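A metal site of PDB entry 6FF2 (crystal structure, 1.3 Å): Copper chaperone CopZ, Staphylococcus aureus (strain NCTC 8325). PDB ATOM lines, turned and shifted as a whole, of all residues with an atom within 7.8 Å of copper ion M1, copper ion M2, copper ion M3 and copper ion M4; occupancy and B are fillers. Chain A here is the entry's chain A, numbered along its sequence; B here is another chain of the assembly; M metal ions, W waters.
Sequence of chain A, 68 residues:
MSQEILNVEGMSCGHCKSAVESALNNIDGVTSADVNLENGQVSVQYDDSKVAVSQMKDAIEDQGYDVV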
ATOM      1  N   GLY A  10      -8.350   0.658 -12.584  1.00  0.00           N
ATOM      2  CA  GLY A  10      -7.923   1.026 -11.223  1.00  0.00           C
ATOM      3  C   GLY A  10      -7.139  -0.064 -10.513  1.00  0.00           C
ATOM      4  O   GLY A  10      -6.629   0.166  -9.422  1.00  0.00           O
ATOM      5  N   MET A  11      -7.031  -1.260 -11.085  1.00  0.00           N
ATOM      6  CA  MET A  11      -6.326  -2.353 -10.385  1.00  0.00           C
ATOM      7  C   MET A  11      -4.846  -2.169 -10.678  1.00  0.00           C
ATOM      8  O   MET A  11      -4.403  -2.300 -11.805  1.00  0.00           O
ATOM      9  CB  MET A  11      -6.801  -3.743 -10.842  1.00  0.00           C
ATOM     10  CG  MET A  11      -8.284  -3.930 -10.644  1.00  0.00           C
ATOM     11  SD  MET A  11      -8.779  -5.598 -11.138  1.00  0.00           S
ATOM     12  CE  MET A  11      -8.320  -5.591 -12.863  1.00  0.00           C
ATOM     13  N   SER A  12      -4.056  -1.853  -9.639  1.00  0.00           N
ATOM     14  CA  SER A  12      -2.657  -1.472  -9.905  1.00  0.00           C
ATOM     15  C   SER A  12      -1.622  -2.420  -9.440  1.00  0.00           C
ATOM     16  O   SER A  12      -0.469  -2.192  -9.740  1.00  0.00           O
ATOM     17  CB  SER A  12      -2.354  -0.102  -9.264  1.00  0.00           C
ATOM     18  OG  SER A  12      -2.613  -0.165  -7.896  1.00  0.00           O
ATOM     19  N   CYS A  13      -1.970  -3.401  -8.637  1.00  0.00           N
ATOM     20  CA  CYS A  13      -0.990  -4.273  -7.985  1.00  0.00           C
ATOM     21  C   CYS A  13      -1.622  -5.556  -7.508  1.00  0.00           C
ATOM     22  O   CYS A  13      -2.823  -5.752  -7.610  1.00  0.00           O
ATOM     23  CB  CYS A  13      -0.341  -3.573  -6.747  1.00  0.00           C
ATOM     24  SG  CYS A  13      -1.433  -3.435  -5.298  1.00  0.00           S
ATOM     25  N   GLY A  14      -0.788  -6.467  -7.000  1.00  0.00           N
ATOM     26  CA  GLY A  14      -1.247  -7.726  -6.431  1.00  0.00           C
ATOM     27  C   GLY A  14      -2.280  -7.642  -5.321  1.00  0.00           C
ATOM     28  O   GLY A  14      -3.116  -8.518  -5.202  1.00  0.00           O
ATOM     29  N   HIS A  15      -2.275  -6.562  -4.521  1.00  0.00           N
ATOM     30  CA  HIS A  15      -3.314  -6.357  -3.510  1.00  0.00           C
ATOM     31  C   HIS A  15      -4.698  -6.114  -4.149  1.00  0.00           C
ATOM     32  O   HIS A  15      -5.714  -6.616  -3.633  1.00  0.00           O
ATOM     33  CB  HIS A  15      -3.007  -5.135  -2.648  1.00  0.00           C
ATOM     34  CG  HIS A  15      -1.826  -5.294  -1.751  1.00  0.00           C
ATOM     35  ND1 HIS A  15      -0.743  -4.448  -1.836  1.00  0.00           N
ATOM     36  CD2 HIS A  15      -1.589  -6.139  -0.726  1.00  0.00           C
ATOM     37  CE1 HIS A  15       0.144  -4.812  -0.914  1.00  0.00           C
ATOM     38  NE2 HIS A  15      -0.356  -5.808  -0.214  1.00  0.00           N
ATOM     39  N   CYS A  16      -4.703  -5.364  -5.258  1.00  0.00           N
ATOM     40  CA  CYS A  16      -5.941  -5.064  -6.000  1.00  0.00           C
ATOM     41  C   CYS A  16      -6.492  -6.377  -6.578  1.00  0.00           C
ATOM     42  O   CYS A  16      -7.687  -6.699  -6.429  1.00  0.00           O
ATOM     43  CB  CYS A  16      -5.718  -4.084  -7.146  1.00  0.00           C
ATOM     44  SG  CYS A  16      -5.256  -2.424  -6.593  1.00  0.00           S
ATOM     45  N   LYS A  17      -5.604  -7.149  -7.172  1.00  0.00           N
ATOM     46  CA  LYS A  17      -5.962  -8.476  -7.703  1.00  0.00           C
ATOM     47  C   LYS A  17      -6.596  -9.330  -6.633  1.00  0.00           C
ATOM     48  O   LYS A  17      -7.652  -9.966  -6.831  1.00  0.00           O
ATOM     49  CB  LYS A  17      -4.778  -9.119  -8.351  1.00  0.00           C
ATOM     50  CG  LYS A  17      -4.870 -10.621  -8.629  1.00  0.00           C
ATOM     51  CD  LYS A  17      -3.720 -10.980  -9.532  1.00  0.00           C
ATOM     52  CE  LYS A  17      -3.569 -12.471  -9.736  1.00  0.00           C
ATOM     53  NZ  LYS A  17      -4.574 -13.008 -10.674  1.00  0.00           N
ATOM     54  N   SER A  18      -5.973  -9.421  -5.475  1.00  0.00           N
ATOM     55  CA  SER A  18      -6.463 -10.260  -4.423  1.00  0.00           C
ATOM     56  C   SER A  18      -7.841  -9.816  -3.963  1.00  0.00           C
ATOM     57  O   SER A  18      -8.742 -10.641  -3.746  1.00  0.00           O
ATOM     58  CB  SER A  18      -5.462 -10.251  -3.290  1.00  0.00           C
ATOM     59  OG  SER A  18      -5.965 -11.033  -2.282  1.00  0.00           O
ATOM     60  N   ALA A  19      -8.016  -8.512  -3.826  1.00  0.00           N
ATOM     61  CA  ALA A  19      -9.271  -7.975  -3.337  1.00  0.00           C
ATOM     62  C   ALA A  19     -10.429  -8.247  -4.321  1.00  0.00           C
ATOM     63  O   ALA A  19     -11.556  -8.507  -3.878  1.00  0.00           O
ATOM     64  CB  ALA A  19      -9.150  -6.477  -3.087  1.00  0.00           C
ATOM     65  N   LEU A  37      -3.689  -8.310 -14.391  1.00  0.00           N
ATOM     66  CA  LEU A  37      -3.340  -6.922 -14.043  1.00  0.00           C
ATOM     67  C   LEU A  37      -2.788  -6.156 -15.224  1.00  0.00           C
ATOM     68  O   LEU A  37      -2.902  -4.935 -15.275  1.00  0.00           O
ATOM     69  CB  LEU A  37      -2.305  -6.885 -12.901  1.00  0.00           C
ATOM     70  CG  LEU A  37      -2.872  -7.213 -11.531  1.00  0.00           C
ATOM     71  CD1 LEU A  37      -1.701  -7.320 -10.562  1.00  0.00           C
ATOM     72  CD2 LEU A  37      -3.875  -6.176 -11.057  1.00  0.00           C
ATOM     73  N   GLN A  63     -15.424  -2.519  -4.088  1.00  0.00           N
ATOM     74  CA  GLN A  63     -13.997  -2.526  -3.720  1.00  0.00           C
ATOM     75  C   GLN A  63     -13.257  -1.281  -4.203  1.00  0.00           C
ATOM     76  O   GLN A  63     -12.047  -1.157  -3.927  1.00  0.00           O
ATOM     77  CB  GLN A  63     -13.278  -3.766  -4.280  1.00  0.00           C
ATOM     78  CG  GLN A  63     -13.784  -5.070  -3.710  1.00  0.00           C
ATOM     79  CD  GLN A  63     -13.504  -5.189  -2.226  1.00  0.00           C
ATOM     80  OE1 GLN A  63     -12.373  -4.956  -1.762  1.00  0.00           O
ATOM     81  NE2 GLN A  63     -14.507  -5.483  -1.464  1.00  0.00           N
ATOM     82  N   TYR A  65     -13.135   0.041  -7.573  1.00  0.00           N
ATOM     83  CA  TYR A  65     -12.661   0.035  -8.975  1.00  0.00           C
ATOM     84  C   TYR A  65     -13.808   0.424  -9.913  1.00  0.00           C
ATOM     85  O   TYR A  65     -14.931   0.434  -9.509  1.00  0.00           O
ATOM     86  CB  TYR A  65     -12.096  -1.388  -9.315  1.00  0.00           C
ATOM     87  CG  TYR A  65     -11.026  -1.787  -8.352  1.00  0.00           C
ATOM     88  CD1 TYR A  65      -9.777  -1.214  -8.415  1.00  0.00           C
ATOM     89  CD2 TYR A  65     -11.280  -2.634  -7.320  1.00  0.00           C
ATOM     90  CE1 TYR A  65      -8.822  -1.497  -7.445  1.00  0.00           C
ATOM     91  CE2 TYR A  65     -10.347  -2.937  -6.361  1.00  0.00           C
ATOM     92  CZ  TYR A  65      -9.135  -2.368  -6.430  1.00  0.00           C
ATOM     93  OH  TYR A  65      -8.269  -2.677  -5.426  1.00  0.00           O
ATOM     94  N   GLY B  10       7.076   1.887  -5.991  1.00  0.00           N
ATOM     95  CA  GLY B  10       6.211   0.727  -6.193  1.00  0.00           C
ATOM     96  C   GLY B  10       4.892   0.782  -5.477  1.00  0.00           C
ATOM     97  O   GLY B  10       4.094  -0.134  -5.618  1.00  0.00           O
ATOM     98  N   MET B  11       4.613   1.846  -4.721  1.00  0.00           N
ATOM     99  CA  MET B  11       3.384   1.911  -3.945  1.00  0.00           C
ATOM    100  C   MET B  11       2.358   2.536  -4.858  1.00  0.00           C
ATOM    101  O   MET B  11       2.461   3.679  -5.235  1.00  0.00           O
ATOM    102  CB  MET B  11       3.521   2.772  -2.697  1.00  0.00           C
ATOM    103  CG  MET B  11       4.568   2.247  -1.716  1.00  0.00           C
ATOM    104  SD  MET B  11       4.715   3.275  -0.240  1.00  0.00           S
ATOM    105  CE  MET B  11       5.123   4.876  -0.939  1.00  0.00           C
ATOM    106  N   SER B  12       1.334   1.785  -5.189  1.00  0.00           N
ATOM    107  CA  SER B  12       0.498   2.227  -6.306  1.00  0.00           C
ATOM    108  C   SER B  12      -0.931   2.523  -5.896  1.00  0.00           C
ATOM    109  O   SER B  12      -1.719   3.006  -6.715  1.00  0.00           O
ATOM    110  CB  SER B  12       0.469   1.149  -7.428  1.00  0.00           C
ATOM    111  OG  SER B  12      -0.064  -0.034  -6.966  1.00  0.00           O
ATOM    112  N   CYS B  13      -1.333   2.175  -4.690  1.00  0.00           N
ATOM    113  CA  CYS B  13      -2.705   2.336  -4.259  1.00  0.00           C
ATOM    114  C   CYS B  13      -2.836   2.339  -2.749  1.00  0.00           C
ATOM    115  O   CYS B  13      -1.868   2.073  -2.036  1.00  0.00           O
ATOM    116  CB  CYS B  13      -3.570   1.187  -4.831  1.00  0.00           C
ATOM    117  SG  CYS B  13      -3.378  -0.404  -4.098  1.00  0.00           S
ATOM    118  N   GLY B  14      -4.047   2.476  -2.293  1.00  0.00           N
ATOM    119  CA  GLY B  14      -4.340   2.483  -0.890  1.00  0.00           C
ATOM    120  C   GLY B  14      -3.971   1.201  -0.198  1.00  0.00           C
ATOM    121  O   GLY B  14      -3.689   1.195   1.003  1.00  0.00           O
ATOM    122  N   HIS B  15      -4.009   0.071  -0.891  1.00  0.00           N
ATOM    123  CA  HIS B  15      -3.616  -1.161  -0.244  1.00  0.00           C
ATOM    124  C   HIS B  15      -2.125  -1.166   0.037  1.00  0.00           C
ATOM    125  O   HIS B  15      -1.678  -1.692   1.094  1.00  0.00           O
ATOM    126  CB  HIS B  15      -3.892  -2.399  -1.144  1.00  0.00           C
ATOM    127  CG  HIS B  15      -5.341  -2.716  -1.350  1.00  0.00           C
ATOM    128  ND1 HIS B  15      -5.923  -2.670  -2.600  1.00  0.00           N
ATOM    129  CD2 HIS B  15      -6.298  -3.098  -0.475  1.00  0.00           C
ATOM    130  CE1 HIS B  15      -7.191  -3.036  -2.488  1.00  0.00           C
ATOM    131  NE2 HIS B  15      -7.454  -3.312  -1.222  1.00  0.00           N
ATOM    132  N   CYS B  16      -1.353  -0.642  -0.908  1.00  0.00           N
ATOM    133  CA  CYS B  16       0.108  -0.528  -0.699  1.00  0.00           C
ATOM    134  C   CYS B  16       0.355   0.407   0.506  1.00  0.00           C
ATOM    135  O   CYS B  16       1.245   0.105   1.330  1.00  0.00           O
ATOM    136  CB  CYS B  16       0.819   0.015  -1.905  1.00  0.00           C
ATOM    137  SG  CYS B  16       0.692  -0.986  -3.405  1.00  0.00           S
ATOM    138  N   LYS B  17      -0.325   1.544   0.540  1.00  0.00           N
ATOM    139  CA  LYS B  17      -0.202   2.475   1.650  1.00  0.00           C
ATOM    140  C   LYS B  17      -0.472   1.800   2.953  1.00  0.00           C
ATOM    141  O   LYS B  17       0.321   1.893   3.938  1.00  0.00           O
ATOM    142  CB  LYS B  17      -1.104   3.655   1.447  1.00  0.00           C
ATOM    143  CG  LYS B  17      -1.320   4.542   2.613  1.00  0.00           C
ATOM    144  CD  LYS B  17      -1.928   5.840   2.102  1.00  0.00           C
ATOM    145  CE  LYS B  17      -2.606   6.543   3.261  1.00  0.00           C
ATOM    146  NZ  LYS B  17      -1.692   7.525   3.838  1.00  0.00           N
ATOM    147  N   SER B  18      -1.576   1.057   3.050  1.00  0.00           N
ATOM    148  CA  SER B  18      -1.906   0.389   4.281  1.00  0.00           C
ATOM    149  C   SER B  18      -0.846  -0.673   4.688  1.00  0.00           C
ATOM    150  O   SER B  18      -0.506  -0.837   5.892  1.00  0.00           O
ATOM    151  CB  SER B  18      -3.302  -0.220   4.085  1.00  0.00           C
ATOM    152  OG  SER B  18      -3.806  -0.806   5.246  1.00  0.00           O
ATOM    153  N   ALA B  19      -0.335  -1.451   3.716  1.00  0.00           N
ATOM    154  CA  ALA B  19       0.676  -2.493   3.947  1.00  0.00           C
ATOM    155  C   ALA B  19       1.946  -1.914   4.549  1.00  0.00           C
ATOM    156  O   ALA B  19       2.488  -2.472   5.494  1.00  0.00           O
ATOM    157  CB  ALA B  19       0.995  -3.290   2.669  1.00  0.00           C
ATOM    158  N   LEU B  37       1.092   8.654  -1.274  1.00  0.00           N
ATOM    159  CA  LEU B  37       1.161   7.963  -2.573  1.00  0.00           C
ATOM    160  C   LEU B  37       1.492   8.847  -3.766  1.00  0.00           C
ATOM    161  O   LEU B  37       2.066   8.362  -4.709  1.00  0.00           O
ATOM    162  CB  LEU B  37      -0.164   7.243  -2.830  1.00  0.00           C
ATOM    163  CG  LEU B  37      -0.447   6.064  -1.917  1.00  0.00           C
ATOM    164  CD1 LEU B  37      -1.896   5.659  -2.108  1.00  0.00           C
ATOM    165  CD2 LEU B  37       0.545   4.929  -2.192  1.00  0.00           C
ATOM    166  N   GLN B  63       7.922  -5.923   2.215  1.00  0.00           N
ATOM    167  CA  GLN B  63       6.605  -5.818   1.638  1.00  0.00           C
ATOM    168  C   GLN B  63       6.595  -5.731   0.131  1.00  0.00           C
ATOM    169  O   GLN B  63       5.492  -5.660  -0.455  1.00  0.00           O
ATOM    170  CB  GLN B  63       5.837  -4.623   2.235  1.00  0.00           C
ATOM    171  CG  GLN B  63       5.487  -4.748   3.714  1.00  0.00           C
ATOM    172  CD  GLN B  63       4.548  -5.868   3.992  1.00  0.00           C
ATOM    173  OE1 GLN B  63       3.487  -5.963   3.384  1.00  0.00           O
ATOM    174  NE2 GLN B  63       4.943  -6.755   4.860  1.00  0.00           N
ATOM    175  N   TYR B  65       8.482  -3.381  -1.853  1.00  0.00           N
ATOM    176  CA  TYR B  65       8.755  -2.051  -2.453  1.00  0.00           C
ATOM    177  C   TYR B  65      10.256  -1.774  -2.423  1.00  0.00           C
ATOM    178  O   TYR B  65      10.978  -2.520  -1.833  1.00  0.00           O
ATOM    179  CB  TYR B  65       7.950  -0.958  -1.724  1.00  0.00           C
ATOM    180  CG  TYR B  65       6.502  -1.344  -1.600  1.00  0.00           C
ATOM    181  CD1 TYR B  65       5.684  -1.304  -2.736  1.00  0.00           C
ATOM    182  CD2 TYR B  65       5.962  -1.894  -0.442  1.00  0.00           C
ATOM    183  CE1 TYR B  65       4.383  -1.727  -2.679  1.00  0.00           C
ATOM    184  CE2 TYR B  65       4.662  -2.328  -0.392  1.00  0.00           C
ATOM    185  CZ  TYR B  65       3.896  -2.233  -1.545  1.00  0.00           C
ATOM    186  OH  TYR B  65       2.623  -2.696  -1.504  1.00  0.00           O
HETATM  187 CU    CU M   1      -3.210  -2.249  -5.760  1.00  0.00          CU
HETATM  188 CU    CU M   2      -0.209  -3.234  -3.344  1.00  0.00          CU
HETATM  189 CU    CU M   3      -5.276  -1.714  -4.256  1.00  0.00          CU
HETATM  190 CU    CU M   4      -1.314  -1.108  -4.288  1.00  0.00          CU
HETATM  191  O   HOH W   1       2.071  -4.357  -4.235  1.00  0.00           O
HETATM  192  O   HOH W   2      -7.061   0.203  -4.538  1.00  0.00           O
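The side-chain sulfur of Cys 16 of chain B lies close to the backbone NH of Ser 12 of chain B, at 3.4 Å. SG of Cys 16 of chain B lies close to OH of Tyr 65 of chain B (3.2 Å). SG of Cys 16 of chain A lies close to N of Ser 12 of chain A (3.3 Å). OH of Tyr 65 of chain A lies close to SG of Cys 16 of chain A, 3.2 Å away. The side-chain hydroxyl (OG) of Ser 12 of chain B lies within hydrogen-bond range of the side-chain hydroxyl (OG) of Ser 12 of chain A.
Merely in contact with copper ion M1: Ser 12 of chain A (3.0 Å). Within 4 Å of copper ion M1: Ser 12 of chain A, Cys 13 of chain A, Cys 16 of chain A and Cys 13 of chain B. The nearest printed residue that does not touch copper ion M1 is Ser 12 of chain B (4.03 Å).
Tyr 65 of chain B touches copper ion M2. Within 4 Å of copper ion M2: Cys 13 of chain A, His 15 of chain A, Cys 16 of chain B and Tyr 65 of chain B. The nearest printed residue that does not touch copper ion M2 is Cys 13 of chain B (4.3 Å).
Residues that only touch copper ion M3: Tyr 65 of chain A. Within 4 Å of copper ion M3: Cys 16 of chain A, Tyr 65 of chain A, Cys 13 of chain B and His 15 of chain B. The nearest printed residue that does not touch copper ion M3 is Cys 13 of chain A (4.3 Å).
Ser 12 of chain A touches copper ion M4 (OG to CU, 3.9 Å). Ser 12 of chain B touches copper ion M4 (OG to CU, 3.1 Å). The nearest printed residue that does not touch copper ion M4 is His 15 of chain A (4.2 Å).
Copper ion M1 is bound by SG of Cys 13 of chain A (2.2 Å). Copper ion M1 is bound by SG of Cys 16 of chain A, 2.2 Å away. The side-chain sulfur (SG) of Cys 13 of chain B binds copper ion M1 (2.5 Å).
Copper ion M2 is bound by ND1 of His 15 of chain A, SG of Cys 13 of chain A and SG of Cys 16 of chain B. Slightly farther from copper ion M2 lies water W1 (2.7 Å).
ND1 of His 15 of chain B binds copper ion M3 (2.0 Å). The side-chain sulfur (SG) of Cys 13 of chain B is bound to copper ion M3 (2.3 Å). The side-chain sulfur (SG) of Cys 16 of chain A is bound to copper ion M3 (2.4 Å). Copper ion M3 has three donor atoms within binding distance. Slightly farther from copper ion M3 lies water W2 (2.6 Å).
Copper ion M4 is bound by SG of Cys 13 of chain B. Copper ion M4 is bound by the side-chain sulfur (SG) of Cys 16 of chain B (2.2 Å). Copper ion M4 is bound by SG of Cys 13 of chain A (2.5 Å). Copper ion M4 has three donor atoms within binding distance.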
